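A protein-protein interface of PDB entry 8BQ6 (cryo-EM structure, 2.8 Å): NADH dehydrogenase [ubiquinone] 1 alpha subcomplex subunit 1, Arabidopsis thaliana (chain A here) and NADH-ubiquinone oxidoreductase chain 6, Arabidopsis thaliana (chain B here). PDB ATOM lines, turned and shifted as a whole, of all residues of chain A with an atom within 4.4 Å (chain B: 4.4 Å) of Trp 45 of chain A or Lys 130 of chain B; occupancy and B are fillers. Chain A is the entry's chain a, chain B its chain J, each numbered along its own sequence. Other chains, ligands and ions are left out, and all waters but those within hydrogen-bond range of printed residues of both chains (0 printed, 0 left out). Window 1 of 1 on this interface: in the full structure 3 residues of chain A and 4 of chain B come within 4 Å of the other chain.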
ATOM      1  N   ASP A  43      16.187  -3.288  32.359  1.00  0.00           N
ATOM      2  CA  ASP A  43      16.089  -4.693  32.684  1.00  0.00           C
ATOM      3  C   ASP A  43      16.588  -5.548  31.518  1.00  0.00           C
ATOM      4  O   ASP A  43      17.133  -5.045  30.528  1.00  0.00           O
ATOM      5  CB  ASP A  43      14.652  -5.026  33.117  1.00  0.00           C
ATOM      6  CG  ASP A  43      13.640  -4.882  31.992  1.00  0.00           C
ATOM      7  OD1 ASP A  43      12.491  -4.475  32.270  1.00  0.00           O
ATOM      8  OD2 ASP A  43      13.976  -5.164  30.833  1.00  0.00           O
ATOM      9  N   GLU A  44      16.405  -6.859  31.663  1.00  0.00           N
ATOM     10  CA  GLU A  44      16.853  -7.821  30.665  1.00  0.00           C
ATOM     11  C   GLU A  44      16.186  -7.569  29.319  1.00  0.00           C
ATOM     12  O   GLU A  44      16.812  -7.736  28.264  1.00  0.00           O
ATOM     13  CB  GLU A  44      16.551  -9.244  31.142  1.00  0.00           C
ATOM     14  CG  GLU A  44      16.933  -9.613  32.595  1.00  0.00           C
ATOM     15  CD  GLU A  44      16.342  -8.702  33.670  1.00  0.00           C
ATOM     16  OE1 GLU A  44      15.113  -8.618  33.784  1.00  0.00           O
ATOM     17  OE2 GLU A  44      17.118  -8.072  34.412  1.00  0.00           O
ATOM     18  N   TRP A  45      14.909  -7.185  29.338  1.00  0.00           N
ATOM     19  CA  TRP A  45      14.211  -6.881  28.095  1.00  0.00           C
ATOM     20  C   TRP A  45      14.864  -5.712  27.373  1.00  0.00           C
ATOM     21  O   TRP A  45      15.116  -5.782  26.170  1.00  0.00           O
ATOM     22  CB  TRP A  45      12.740  -6.577  28.379  1.00  0.00           C
ATOM     23  CG  TRP A  45      11.946  -6.239  27.160  1.00  0.00           C
ATOM     24  CD1 TRP A  45      11.815  -5.011  26.589  1.00  0.00           C
ATOM     25  CD2 TRP A  45      11.149  -7.133  26.375  1.00  0.00           C
ATOM     26  NE1 TRP A  45      10.997  -5.083  25.491  1.00  0.00           N
ATOM     27  CE2 TRP A  45      10.572  -6.376  25.339  1.00  0.00           C
ATOM     28  CE3 TRP A  45      10.868  -8.499  26.448  1.00  0.00           C
ATOM     29  CZ2 TRP A  45       9.735  -6.937  24.382  1.00  0.00           C
ATOM     30  CZ3 TRP A  45      10.036  -9.053  25.497  1.00  0.00           C
ATOM     31  CH2 TRP A  45       9.480  -8.274  24.477  1.00  0.00           C
ATOM     32  N   ASP A  46      15.135  -4.623  28.095  1.00  0.00           N
ATOM     33  CA  ASP A  46      15.736  -3.447  27.469  1.00  0.00           C
ATOM     34  C   ASP A  46      17.131  -3.751  26.949  1.00  0.00           C
ATOM     35  O   ASP A  46      17.530  -3.255  25.887  1.00  0.00           O
ATOM     36  CB  ASP A  46      15.781  -2.297  28.466  1.00  0.00           C
ATOM     37  CG  ASP A  46      14.416  -1.925  28.968  1.00  0.00           C
ATOM     38  OD1 ASP A  46      14.217  -1.900  30.198  1.00  0.00           O
ATOM     39  OD2 ASP A  46      13.537  -1.665  28.127  1.00  0.00           O
ATOM     40  N   VAL A  47      17.890  -4.555  27.690  1.00  0.00           N
ATOM     41  CA  VAL A  47      19.207  -4.970  27.224  1.00  0.00           C
ATOM     42  C   VAL A  47      19.085  -5.765  25.930  1.00  0.00           C
ATOM     43  O   VAL A  47      19.817  -5.520  24.959  1.00  0.00           O
ATOM     44  CB  VAL A  47      19.922  -5.770  28.330  1.00  0.00           C
ATOM     45  CG1 VAL A  47      21.194  -6.383  27.805  1.00  0.00           C
ATOM     46  CG2 VAL A  47      20.224  -4.869  29.516  1.00  0.00           C
ATOM     47  N   ALA A  48      18.145  -6.711  25.884  1.00  0.00           N
ATOM     48  CA  ALA A  48      17.954  -7.514  24.681  1.00  0.00           C
ATOM     49  C   ALA A  48      17.461  -6.663  23.516  1.00  0.00           C
ATOM     50  O   ALA A  48      17.820  -6.912  22.360  1.00  0.00           O
ATOM     51  CB  ALA A  48      16.979  -8.655  24.967  1.00  0.00           C
ATOM     52  N   MET A  49      16.634  -5.655  23.802  1.00  0.00           N
ATOM     53  CA  MET A  49      16.164  -4.747  22.761  1.00  0.00           C
ATOM     54  C   MET A  49      17.313  -3.937  22.190  1.00  0.00           C
ATOM     55  O   MET A  49      17.375  -3.696  20.984  1.00  0.00           O
ATOM     56  CB  MET A  49      15.088  -3.808  23.303  1.00  0.00           C
ATOM     57  CG  MET A  49      13.786  -4.469  23.694  1.00  0.00           C
ATOM     58  SD  MET A  49      12.809  -5.036  22.298  1.00  0.00           S
ATOM     59  CE  MET A  49      13.389  -6.724  22.176  1.00  0.00           C
ATOM     60  N   THR B 125      17.699 -16.957  22.196  1.00  0.00           N
ATOM     61  CA  THR B 125      17.019 -16.054  23.114  1.00  0.00           C
ATOM     62  C   THR B 125      15.525 -16.345  23.099  1.00  0.00           C
ATOM     63  O   THR B 125      14.913 -16.405  22.028  1.00  0.00           O
ATOM     64  CB  THR B 125      17.270 -14.590  22.742  1.00  0.00           C
ATOM     65  OG1 THR B 125      18.644 -14.264  22.977  1.00  0.00           O
ATOM     66  CG2 THR B 125      16.399 -13.668  23.578  1.00  0.00           C
ATOM     67  N   VAL B 126      14.946 -16.529  24.282  1.00  0.00           N
ATOM     68  CA  VAL B 126      13.507 -16.697  24.447  1.00  0.00           C
ATOM     69  C   VAL B 126      12.983 -15.446  25.136  1.00  0.00           C
ATOM     70  O   VAL B 126      13.218 -15.242  26.334  1.00  0.00           O
ATOM     71  CB  VAL B 126      13.161 -17.958  25.247  1.00  0.00           C
ATOM     72  CG1 VAL B 126      11.662 -18.048  25.464  1.00  0.00           C
ATOM     73  CG2 VAL B 126      13.672 -19.193  24.533  1.00  0.00           C
ATOM     74  N   TYR B 127      12.262 -14.611  24.393  1.00  0.00           N
ATOM     75  CA  TYR B 127      11.837 -13.331  24.938  1.00  0.00           C
ATOM     76  C   TYR B 127      10.679 -13.453  25.920  1.00  0.00           C
ATOM     77  O   TYR B 127      10.439 -12.512  26.683  1.00  0.00           O
ATOM     78  CB  TYR B 127      11.437 -12.380  23.814  1.00  0.00           C
ATOM     79  CG  TYR B 127      12.557 -11.948  22.913  1.00  0.00           C
ATOM     80  CD1 TYR B 127      13.400 -10.910  23.276  1.00  0.00           C
ATOM     81  CD2 TYR B 127      12.755 -12.556  21.684  1.00  0.00           C
ATOM     82  CE1 TYR B 127      14.421 -10.503  22.451  1.00  0.00           C
ATOM     83  CE2 TYR B 127      13.771 -12.157  20.852  1.00  0.00           C
ATOM     84  CZ  TYR B 127      14.603 -11.130  21.240  1.00  0.00           C
ATOM     85  OH  TYR B 127      15.621 -10.726  20.411  1.00  0.00           O
ATOM     86  N   ALA B 128       9.964 -14.579  25.920  1.00  0.00           N
ATOM     87  CA  ALA B 128       8.814 -14.722  26.808  1.00  0.00           C
ATOM     88  C   ALA B 128       9.226 -14.623  28.271  1.00  0.00           C
ATOM     89  O   ALA B 128       8.518 -14.018  29.084  1.00  0.00           O
ATOM     90  CB  ALA B 128       8.104 -16.047  26.539  1.00  0.00           C
ATOM     91  N   GLY B 129      10.368 -15.203  28.626  1.00  0.00           N
ATOM     92  CA  GLY B 129      10.852 -15.087  29.987  1.00  0.00           C
ATOM     93  C   GLY B 129      11.271 -13.694  30.407  1.00  0.00           C
ATOM     94  O   GLY B 129      11.407 -13.444  31.608  1.00  0.00           O
ATOM     95  N   LYS B 130      11.468 -12.778  29.460  1.00  0.00           N
ATOM     96  CA  LYS B 130      12.015 -11.456  29.734  1.00  0.00           C
ATOM     97  C   LYS B 130      10.961 -10.369  29.876  1.00  0.00           C
ATOM     98  O   LYS B 130      11.325  -9.207  30.083  1.00  0.00           O
ATOM     99  CB  LYS B 130      12.982 -11.055  28.622  1.00  0.00           C
ATOM    100  CG  LYS B 130      14.333 -11.694  28.705  1.00  0.00           C
ATOM    101  CD  LYS B 130      15.060 -11.543  27.391  1.00  0.00           C
ATOM    102  CE  LYS B 130      16.486 -12.021  27.520  1.00  0.00           C
ATOM    103  NZ  LYS B 130      16.529 -13.460  27.892  1.00  0.00           N
ATOM    104  N   VAL B 131       9.676 -10.702  29.748  1.00  0.00           N
ATOM    105  CA  VAL B 131       8.636  -9.677  29.805  1.00  0.00           C
ATOM    106  C   VAL B 131       8.556  -9.064  31.197  1.00  0.00           C
ATOM    107  O   VAL B 131       8.557  -7.836  31.352  1.00  0.00           O
ATOM    108  CB  VAL B 131       7.284 -10.271  29.375  1.00  0.00           C
ATOM    109  CG1 VAL B 131       6.153  -9.331  29.745  1.00  0.00           C
ATOM    110  CG2 VAL B 131       7.276 -10.550  27.887  1.00  0.00           C
ATOM    111  N   ARG B 132       8.472  -9.907  32.226  1.00  0.00           N
ATOM    112  CA  ARG B 132       8.443  -9.488  33.631  1.00  0.00           C
ATOM    113  C   ARG B 132       9.414 -10.412  34.359  1.00  0.00           C
ATOM    114  O   ARG B 132       9.034 -11.492  34.818  1.00  0.00           O
ATOM    115  CB  ARG B 132       7.039  -9.567  34.223  1.00  0.00           C
ATOM    116  CG  ARG B 132       6.958  -9.185  35.702  1.00  0.00           C
ATOM    117  CD  ARG B 132       5.547  -9.356  36.260  1.00  0.00           C
ATOM    118  NE  ARG B 132       5.478  -9.080  37.692  1.00  0.00           N
ATOM    119  CZ  ARG B 132       4.348  -8.967  38.377  1.00  0.00           C
ATOM    120  NH1 ARG B 132       3.169  -9.131  37.800  1.00  0.00           N
ATOM    121  NH2 ARG B 132       4.402  -8.671  39.674  1.00  0.00           N
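Of the 7 printed residues of chain A, 2 touch a printed residue of chain B. Among the printed residues, no Asp or Glu carboxylate lies within 4 Å of a Lys or Arg side-chain nitrogen of the other chain.
Trp 45 of chain A touches just these residues of chain B: Tyr 127 (3.7 Å), Lys 130 (3.4 Å) and Val 131 (3.9 Å). Of chain A, only Trp 45 comes within 4 Å of Lys 130 of chain B. Of the printed residues of chain B, Met 49 of chain A touches Tyr 127 (3.9 Å). Of the printed residues of chain A, Tyr 127 of chain B touches Trp 45 and Met 49. Of the printed residues of chain A, Val 131 of chain B touches Trp 45. The nearest printed residue of chain A that does not touch Tyr 127 of chain B is Ala 48 of chain A (4.04 Å).
The side-chain carboxylate (OD2) of Asp 43 of chain A sits at hydrogen-bond distance from the backbone NH (N) of Trp 45 of chain A (2.7 Å). SD of Met 49 of chain A sits close to NE1 of Trp 45 of chain A, at 3.7 Å.
Tyr 127 of chain B touches Trp 45 of chain A (O to CZ3, 3.7 Å). Trp 45 of chain A touches Lys 130 of chain B (CB to O, 3.4 Å). CZ3 of Trp 45 of chain A touches CG2 of Val 131 of chain B, 3.9 Å away. Tyr 127 of chain B touches Met 49 of chain A.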
